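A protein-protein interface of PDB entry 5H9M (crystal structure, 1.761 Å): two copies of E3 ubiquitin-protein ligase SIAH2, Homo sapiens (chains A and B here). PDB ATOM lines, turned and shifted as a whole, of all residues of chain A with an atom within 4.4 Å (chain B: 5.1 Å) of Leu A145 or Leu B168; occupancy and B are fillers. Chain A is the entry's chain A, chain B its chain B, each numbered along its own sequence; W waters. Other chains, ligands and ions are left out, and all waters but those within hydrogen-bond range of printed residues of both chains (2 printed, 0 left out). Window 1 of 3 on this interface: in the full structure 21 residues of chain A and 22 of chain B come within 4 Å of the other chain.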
ATOM      1  N   LEU A 136     -11.628 -40.921 -16.648  1.00  0.00           N
ATOM      2  CA  LEU A 136     -10.727 -40.553 -17.726  1.00  0.00           C
ATOM      3  C   LEU A 136      -9.755 -39.487 -17.241  1.00  0.00           C
ATOM      4  O   LEU A 136     -10.189 -38.493 -16.651  1.00  0.00           O
ATOM      5  CB  LEU A 136     -11.498 -39.988 -18.910  1.00  0.00           C
ATOM      6  CG  LEU A 136     -12.562 -40.865 -19.543  1.00  0.00           C
ATOM      7  CD1 LEU A 136     -13.273 -40.131 -20.680  1.00  0.00           C
ATOM      8  CD2 LEU A 136     -11.935 -42.159 -20.047  1.00  0.00           C
ATOM      9  N   GLU A 137      -8.463 -39.680 -17.490  1.00  0.00           N
ATOM     10  CA  GLU A 137      -7.425 -38.690 -17.120  1.00  0.00           C
ATOM     11  C   GLU A 137      -6.558 -38.349 -18.310  1.00  0.00           C
ATOM     12  O   GLU A 137      -6.133 -39.234 -19.048  1.00  0.00           O
ATOM     13  CB  GLU A 137      -6.455 -39.199 -16.069  1.00  0.00           C
ATOM     14  CG  GLU A 137      -7.050 -39.694 -14.761  1.00  0.00           C
ATOM     15  CD  GLU A 137      -5.970 -40.117 -13.774  1.00  0.00           C
ATOM     16  OE1 GLU A 137      -4.796 -40.269 -14.182  1.00  0.00           O
ATOM     17  OE2 GLU A 137      -6.289 -40.284 -12.571  1.00  0.00           O
ATOM     18  N   LEU A 138      -6.274 -37.074 -18.461  1.00  0.00           N
ATOM     19  CA  LEU A 138      -5.177 -36.605 -19.312  1.00  0.00           C
ATOM     20  C   LEU A 138      -4.085 -36.209 -18.336  1.00  0.00           C
ATOM     21  O   LEU A 138      -4.339 -35.471 -17.402  1.00  0.00           O
ATOM     22  CB  LEU A 138      -5.615 -35.413 -20.128  1.00  0.00           C
ATOM     23  CG  LEU A 138      -6.851 -35.574 -21.009  1.00  0.00           C
ATOM     24  CD1 LEU A 138      -6.942 -34.371 -21.936  1.00  0.00           C
ATOM     25  CD2 LEU A 138      -6.811 -36.870 -21.803  1.00  0.00           C
ATOM     26  N   ARG A 144      -3.135 -32.419 -14.516  1.00  0.00           N
ATOM     27  CA  ARG A 144      -4.078 -33.536 -14.768  1.00  0.00           C
ATOM     28  C   ARG A 144      -5.485 -32.987 -14.922  1.00  0.00           C
ATOM     29  O   ARG A 144      -5.937 -32.208 -14.097  1.00  0.00           O
ATOM     30  CB  ARG A 144      -4.018 -34.623 -13.673  1.00  0.00           C
ATOM     31  CG  ARG A 144      -4.955 -35.776 -13.955  1.00  0.00           C
ATOM     32  CD  ARG A 144      -5.109 -36.731 -12.782  1.00  0.00           C
ATOM     33  NE  ARG A 144      -3.845 -37.418 -12.538  1.00  0.00           N
ATOM     34  CZ  ARG A 144      -3.062 -37.267 -11.469  1.00  0.00           C
ATOM     35  NH1 ARG A 144      -3.365 -36.451 -10.467  1.00  0.00           N
ATOM     36  NH2 ARG A 144      -1.944 -37.970 -11.396  1.00  0.00           N
ATOM     37  N   LEU A 145      -6.162 -33.392 -16.000  1.00  0.00           N
ATOM     38  CA  LEU A 145      -7.573 -33.168 -16.208  1.00  0.00           C
ATOM     39  C   LEU A 145      -8.283 -34.513 -16.032  1.00  0.00           C
ATOM     40  O   LEU A 145      -7.898 -35.496 -16.668  1.00  0.00           O
ATOM     41  CB  LEU A 145      -7.812 -32.640 -17.632  1.00  0.00           C
ATOM     42  CG  LEU A 145      -9.264 -32.378 -18.045  1.00  0.00           C
ATOM     43  CD1 LEU A 145      -9.926 -31.350 -17.133  1.00  0.00           C
ATOM     44  CD2 LEU A 145      -9.312 -31.903 -19.478  1.00  0.00           C
ATOM     45  N   THR A 146      -9.325 -34.555 -15.203  1.00  0.00           N
ATOM     46  CA  THR A 146     -10.042 -35.802 -14.902  1.00  0.00           C
ATOM     47  C   THR A 146     -11.544 -35.637 -15.045  1.00  0.00           C
ATOM     48  O   THR A 146     -12.096 -34.666 -14.552  1.00  0.00           O
ATOM     49  CB  THR A 146      -9.795 -36.274 -13.461  1.00  0.00           C
ATOM     50  OG1 THR A 146      -8.389 -36.273 -13.179  1.00  0.00           O
ATOM     51  CG2 THR A 146     -10.346 -37.647 -13.235  1.00  0.00           C
ATOM     52  N   LEU A 168     -15.944 -36.277 -21.077  1.00  0.00           N
ATOM     53  CA  LEU A 168     -14.742 -35.465 -20.982  1.00  0.00           C
ATOM     54  C   LEU A 168     -14.703 -34.617 -22.257  1.00  0.00           C
ATOM     55  O   LEU A 168     -14.792 -35.176 -23.344  1.00  0.00           O
ATOM     56  CB  LEU A 168     -13.479 -36.319 -20.881  1.00  0.00           C
ATOM     57  CG  LEU A 168     -12.127 -35.581 -20.976  1.00  0.00           C
ATOM     58  CD1 LEU A 168     -11.963 -34.581 -19.849  1.00  0.00           C
ATOM     59  CD2 LEU A 168     -10.935 -36.531 -21.024  1.00  0.00           C
ATOM     60  N   ILE A 174      -5.783 -27.799 -25.391  1.00  0.00           N
ATOM     61  CA  ILE A 174      -5.642 -28.681 -24.248  1.00  0.00           C
ATOM     62  C   ILE A 174      -4.937 -29.962 -24.661  1.00  0.00           C
ATOM     63  O   ILE A 174      -4.024 -30.414 -23.981  1.00  0.00           O
ATOM     64  CB  ILE A 174      -7.016 -29.011 -23.623  1.00  0.00           C
ATOM     65  CG1 ILE A 174      -7.700 -27.735 -23.088  1.00  0.00           C
ATOM     66  CG2 ILE A 174      -6.877 -30.096 -22.555  1.00  0.00           C
ATOM     67  CD1 ILE A 174      -9.230 -27.730 -23.130  1.00  0.00           C
ATOM     68  N   PHE A 178      -1.149 -32.127 -23.339  1.00  0.00           N
ATOM     69  CA  PHE A 178      -1.081 -33.512 -22.886  1.00  0.00           C
ATOM     70  C   PHE A 178      -0.585 -34.536 -23.914  1.00  0.00           C
ATOM     71  O   PHE A 178      -0.317 -35.666 -23.552  1.00  0.00           O
ATOM     72  CB  PHE A 178      -2.467 -33.894 -22.383  1.00  0.00           C
ATOM     73  CG  PHE A 178      -2.891 -33.132 -21.160  1.00  0.00           C
ATOM     74  CD1 PHE A 178      -2.315 -33.437 -19.935  1.00  0.00           C
ATOM     75  CD2 PHE A 178      -3.882 -32.166 -21.215  1.00  0.00           C
ATOM     76  CE1 PHE A 178      -2.705 -32.762 -18.777  1.00  0.00           C
ATOM     77  CE2 PHE A 178      -4.274 -31.474 -20.060  1.00  0.00           C
ATOM     78  CZ  PHE A 178      -3.686 -31.796 -18.846  1.00  0.00           C
ATOM     79  N   PHE B 116     -16.397 -21.499 -19.607  1.00  0.00           N
ATOM     80  CA  PHE B 116     -15.888 -21.173 -18.271  1.00  0.00           C
ATOM     81  C   PHE B 116     -14.422 -21.599 -18.139  1.00  0.00           C
ATOM     82  O   PHE B 116     -14.041 -22.674 -18.611  1.00  0.00           O
ATOM     83  CB  PHE B 116     -16.693 -21.900 -17.214  1.00  0.00           C
ATOM     84  CG  PHE B 116     -18.080 -21.348 -17.030  1.00  0.00           C
ATOM     85  CD1 PHE B 116     -19.128 -21.756 -17.855  1.00  0.00           C
ATOM     86  CD2 PHE B 116     -18.337 -20.416 -16.034  1.00  0.00           C
ATOM     87  CE1 PHE B 116     -20.404 -21.221 -17.692  1.00  0.00           C
ATOM     88  CE2 PHE B 116     -19.625 -19.896 -15.846  1.00  0.00           C
ATOM     89  CZ  PHE B 116     -20.658 -20.303 -16.684  1.00  0.00           C
ATOM     90  N   PHE B 117     -13.640 -20.754 -17.476  1.00  0.00           N
ATOM     91  CA  PHE B 117     -12.209 -20.961 -17.232  1.00  0.00           C
ATOM     92  C   PHE B 117     -11.958 -20.777 -15.746  1.00  0.00           C
ATOM     93  O   PHE B 117     -12.332 -19.749 -15.195  1.00  0.00           O
ATOM     94  CB  PHE B 117     -11.402 -19.966 -18.044  1.00  0.00           C
ATOM     95  CG  PHE B 117     -11.673 -20.073 -19.503  1.00  0.00           C
ATOM     96  CD1 PHE B 117     -12.779 -19.441 -20.059  1.00  0.00           C
ATOM     97  CD2 PHE B 117     -10.861 -20.852 -20.315  1.00  0.00           C
ATOM     98  CE1 PHE B 117     -13.074 -19.577 -21.400  1.00  0.00           C
ATOM     99  CE2 PHE B 117     -11.149 -20.979 -21.671  1.00  0.00           C
ATOM    100  CZ  PHE B 117     -12.254 -20.342 -22.213  1.00  0.00           C
ATOM    101  N   ALA B 118     -11.349 -21.762 -15.099  1.00  0.00           N
ATOM    102  CA  ALA B 118     -11.089 -21.665 -13.654  1.00  0.00           C
ATOM    103  C   ALA B 118      -9.616 -21.903 -13.370  1.00  0.00           C
ATOM    104  O   ALA B 118      -8.999 -22.846 -13.900  1.00  0.00           O
ATOM    105  CB  ALA B 118     -11.946 -22.653 -12.895  1.00  0.00           C
ATOM    106  N   LEU B 136      -8.965 -28.312  -8.371  1.00  0.00           N
ATOM    107  CA  LEU B 136     -10.321 -27.754  -8.538  1.00  0.00           C
ATOM    108  C   LEU B 136     -11.241 -28.891  -8.882  1.00  0.00           C
ATOM    109  O   LEU B 136     -10.912 -29.680  -9.764  1.00  0.00           O
ATOM    110  CB  LEU B 136     -10.378 -26.766  -9.689  1.00  0.00           C
ATOM    111  CG  LEU B 136      -9.414 -25.617  -9.620  1.00  0.00           C
ATOM    112  CD1 LEU B 136      -9.447 -24.831 -10.930  1.00  0.00           C
ATOM    113  CD2 LEU B 136      -9.693 -24.724  -8.418  1.00  0.00           C
ATOM    114  N   LEU B 138     -15.387 -29.942  -9.565  1.00  0.00           N
ATOM    115  CA  LEU B 138     -16.831 -29.760  -9.695  1.00  0.00           C
ATOM    116  C   LEU B 138     -17.419 -31.121  -9.334  1.00  0.00           C
ATOM    117  O   LEU B 138     -17.070 -32.119  -9.960  1.00  0.00           O
ATOM    118  CB  LEU B 138     -17.218 -29.403 -11.117  1.00  0.00           C
ATOM    119  CG  LEU B 138     -16.634 -28.178 -11.824  1.00  0.00           C
ATOM    120  CD1 LEU B 138     -17.360 -27.937 -13.135  1.00  0.00           C
ATOM    121  CD2 LEU B 138     -16.710 -26.938 -10.980  1.00  0.00           C
ATOM    122  N   LEU B 145     -15.612 -33.424 -12.218  1.00  0.00           N
ATOM    123  CA  LEU B 145     -14.633 -32.862 -13.156  1.00  0.00           C
ATOM    124  C   LEU B 145     -13.559 -32.205 -12.328  1.00  0.00           C
ATOM    125  O   LEU B 145     -13.857 -31.351 -11.492  1.00  0.00           O
ATOM    126  CB  LEU B 145     -15.295 -31.855 -14.092  1.00  0.00           C
ATOM    127  CG  LEU B 145     -14.386 -31.093 -15.053  1.00  0.00           C
ATOM    128  CD1 LEU B 145     -13.721 -32.044 -16.024  1.00  0.00           C
ATOM    129  CD2 LEU B 145     -15.166 -29.974 -15.769  1.00  0.00           C
ATOM    130  N   THR B 146     -12.313 -32.614 -12.552  1.00  0.00           N
ATOM    131  CA  THR B 146     -11.187 -32.199 -11.721  1.00  0.00           C
ATOM    132  C   THR B 146     -10.014 -31.665 -12.579  1.00  0.00           C
ATOM    133  O   THR B 146      -9.690 -32.216 -13.629  1.00  0.00           O
ATOM    134  CB  THR B 146     -10.652 -33.385 -10.883  1.00  0.00           C
ATOM    135  OG1 THR B 146     -11.731 -34.034 -10.184  1.00  0.00           O
ATOM    136  CG2 THR B 146      -9.648 -32.904  -9.867  1.00  0.00           C
ATOM    137  N   TRP B 147      -9.389 -30.605 -12.089  1.00  0.00           N
ATOM    138  CA  TRP B 147      -8.164 -30.044 -12.620  1.00  0.00           C
ATOM    139  C   TRP B 147      -7.160 -29.997 -11.461  1.00  0.00           C
ATOM    140  O   TRP B 147      -7.481 -29.511 -10.366  1.00  0.00           O
ATOM    141  CB  TRP B 147      -8.428 -28.640 -13.170  1.00  0.00           C
ATOM    142  CG  TRP B 147      -7.221 -27.918 -13.679  1.00  0.00           C
ATOM    143  CD1 TRP B 147      -6.574 -26.868 -13.069  1.00  0.00           C
ATOM    144  CD2 TRP B 147      -6.512 -28.172 -14.886  1.00  0.00           C
ATOM    145  NE1 TRP B 147      -5.500 -26.483 -13.821  1.00  0.00           N
ATOM    146  CE2 TRP B 147      -5.439 -27.251 -14.948  1.00  0.00           C
ATOM    147  CE3 TRP B 147      -6.681 -29.077 -15.938  1.00  0.00           C
ATOM    148  CZ2 TRP B 147      -4.540 -27.210 -16.018  1.00  0.00           C
ATOM    149  CZ3 TRP B 147      -5.781 -29.022 -17.008  1.00  0.00           C
ATOM    150  CH2 TRP B 147      -4.723 -28.102 -17.029  1.00  0.00           C
ATOM    151  N   ASP B 166      -4.429 -23.272 -20.116  1.00  0.00           N
ATOM    152  CA  ASP B 166      -3.646 -23.892 -19.056  1.00  0.00           C
ATOM    153  C   ASP B 166      -4.358 -23.648 -17.721  1.00  0.00           C
ATOM    154  O   ASP B 166      -3.890 -22.956 -16.830  1.00  0.00           O
ATOM    155  CB  ASP B 166      -2.227 -23.345 -19.080  1.00  0.00           C
ATOM    156  CG  ASP B 166      -1.256 -24.167 -18.253  1.00  0.00           C
ATOM    157  OD1 ASP B 166      -1.633 -25.195 -17.611  1.00  0.00           O
ATOM    158  OD2 ASP B 166      -0.078 -23.777 -18.271  1.00  0.00           O
ATOM    159  N   CYS B 167      -5.542 -24.241 -17.632  1.00  0.00           N
ATOM    160  CA  CYS B 167      -6.492 -24.027 -16.538  1.00  0.00           C
ATOM    161  C   CYS B 167      -7.614 -25.027 -16.773  1.00  0.00           C
ATOM    162  O   CYS B 167      -7.597 -25.748 -17.763  1.00  0.00           O
ATOM    163  CB  CYS B 167      -7.025 -22.609 -16.572  1.00  0.00           C
ATOM    164  SG  CYS B 167      -7.894 -22.149 -18.080  1.00  0.00           S
ATOM    165  N   LEU B 168      -8.595 -25.070 -15.883  1.00  0.00           N
ATOM    166  CA  LEU B 168      -9.781 -25.883 -16.106  1.00  0.00           C
ATOM    167  C   LEU B 168     -10.691 -25.156 -17.083  1.00  0.00           C
ATOM    168  O   LEU B 168     -11.069 -24.021 -16.833  1.00  0.00           O
ATOM    169  CB  LEU B 168     -10.531 -26.117 -14.811  1.00  0.00           C
ATOM    170  CG  LEU B 168     -11.788 -26.960 -14.956  1.00  0.00           C
ATOM    171  CD1 LEU B 168     -11.536 -28.333 -15.546  1.00  0.00           C
ATOM    172  CD2 LEU B 168     -12.437 -27.060 -13.590  1.00  0.00           C
ATOM    173  N   VAL B 169     -11.044 -25.825 -18.178  1.00  0.00           N
ATOM    174  CA  VAL B 169     -11.918 -25.248 -19.212  1.00  0.00           C
ATOM    175  C   VAL B 169     -13.174 -26.096 -19.319  1.00  0.00           C
ATOM    176  O   VAL B 169     -13.093 -27.310 -19.496  1.00  0.00           O
ATOM    177  CB  VAL B 169     -11.238 -25.219 -20.590  1.00  0.00           C
ATOM    178  CG1 VAL B 169     -12.133 -24.562 -21.616  1.00  0.00           C
ATOM    179  CG2 VAL B 169      -9.867 -24.532 -20.522  1.00  0.00           C
ATOM    180  N   PHE B 170     -14.346 -25.469 -19.260  1.00  0.00           N
ATOM    181  CA  PHE B 170     -15.565 -26.235 -19.415  1.00  0.00           C
ATOM    182  C   PHE B 170     -16.678 -25.504 -20.097  1.00  0.00           C
ATOM    183  O   PHE B 170     -16.808 -24.319 -19.959  1.00  0.00           O
ATOM    184  CB  PHE B 170     -16.044 -26.882 -18.094  1.00  0.00           C
ATOM    185  CG  PHE B 170     -16.233 -25.933 -16.935  1.00  0.00           C
ATOM    186  CD1 PHE B 170     -15.132 -25.493 -16.194  1.00  0.00           C
ATOM    187  CD2 PHE B 170     -17.500 -25.562 -16.513  1.00  0.00           C
ATOM    188  CE1 PHE B 170     -15.289 -24.664 -15.108  1.00  0.00           C
ATOM    189  CE2 PHE B 170     -17.669 -24.740 -15.403  1.00  0.00           C
ATOM    190  CZ  PHE B 170     -16.560 -24.278 -14.704  1.00  0.00           C
HETATM  191  O   HOH W   1     -12.811 -36.113 -11.630  1.00  0.00           O
HETATM  192  O   HOH W   2      -7.382 -34.009 -12.138  1.00  0.00           O
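Among the printed residues, pairs that only touch across the chains: Arg A144 with Thr B146, Arg A144 with Trp B147, Leu A145 with Thr B146, Leu A145 with Leu B168, Thr A146 with Leu B145 and Phe A178 with Trp B147.
Leu A145 touches Thr B146, and with the chains exchanged Thr A146 touches Leu B145.
Leu A145 touches Leu B168, but with the chains exchanged Leu A168 does not touch Leu B145 (4.9 Å).
Thr B146 touches its own counterpart, Thr A146.
5 positions are printed for both chains.
Hydrophobic or aromatic side chains of chain B that line the printed part of chain A: Leu B145, Trp B147 and Leu B168.
Printed residues of chain A that touch a printed residue of chain B: Arg A144, Leu A145, Thr A146 and Phe A178.
Hydrophobic or aromatic side chains of chain A that line the printed part of chain B: Leu A145 and Phe A178.
Among the printed residues, 7 pairs touch across the chains.
Among the printed residues, no Asp or Glu carboxylate lies within 4 Å of a Lys or Arg side-chain nitrogen of the other chain.
The backbone NH (N) of Thr A146 is in hydrogen-bond range of the backbone carbonyl oxygen (O) of Thr B146, 2.8 Å away.
The guanidinium group (NE) of Arg A144 is in salt-bridge range of the side-chain carboxylate (OE1) of Glu A137 (3.4 Å).
The backbone carbonyl oxygen (O) of Leu A145 sits at hydrogen-bond distance from the backbone NH (N) of Leu A138 (2.9 Å).
N of Ala B118 is in hydrogen-bond range of O of Leu B168 (2.9 Å).
The backbone NH of Leu B136 lies within hydrogen-bond range of the backbone carbonyl oxygen of Trp B147 (2.8 Å).
The backbone carbonyl oxygen (O) of Leu B145 lies within hydrogen-bond range of the backbone NH (N) of Leu B138.
Of the printed residues of chain B, Leu A145 touches Thr B146 and Leu B168.
Leu B168 touches one residue of chain A.
Of the printed residues of chain B, Thr A146 touches Leu B145 (3.4 Å) and Thr B146 (2.8 Å).
Printed residues of chain B within 4 Å of Arg A144: Thr B146 and Trp B147.
Leu A136 touches none of the printed residues of chain B.
The nearest printed residue of chain B that does not touch Leu A145 is Leu B145 (4.01 Å).
The nearest printed residue of chain A that does not touch Leu B168 is Thr A146 (6.4 Å).
The nearest printed residue of chain B that does not touch Thr A146 is Trp B147 (5.0 Å).
Water W2 lies within hydrogen-bond range of OG1 of Thr A146, O of Arg A144 and O of Thr B146.
Water W1 lies within hydrogen-bond range of the side-chain hydroxyl of Thr B146 (2.8 Å) and the backbone carbonyl oxygen of Thr A146 (3.3 Å).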
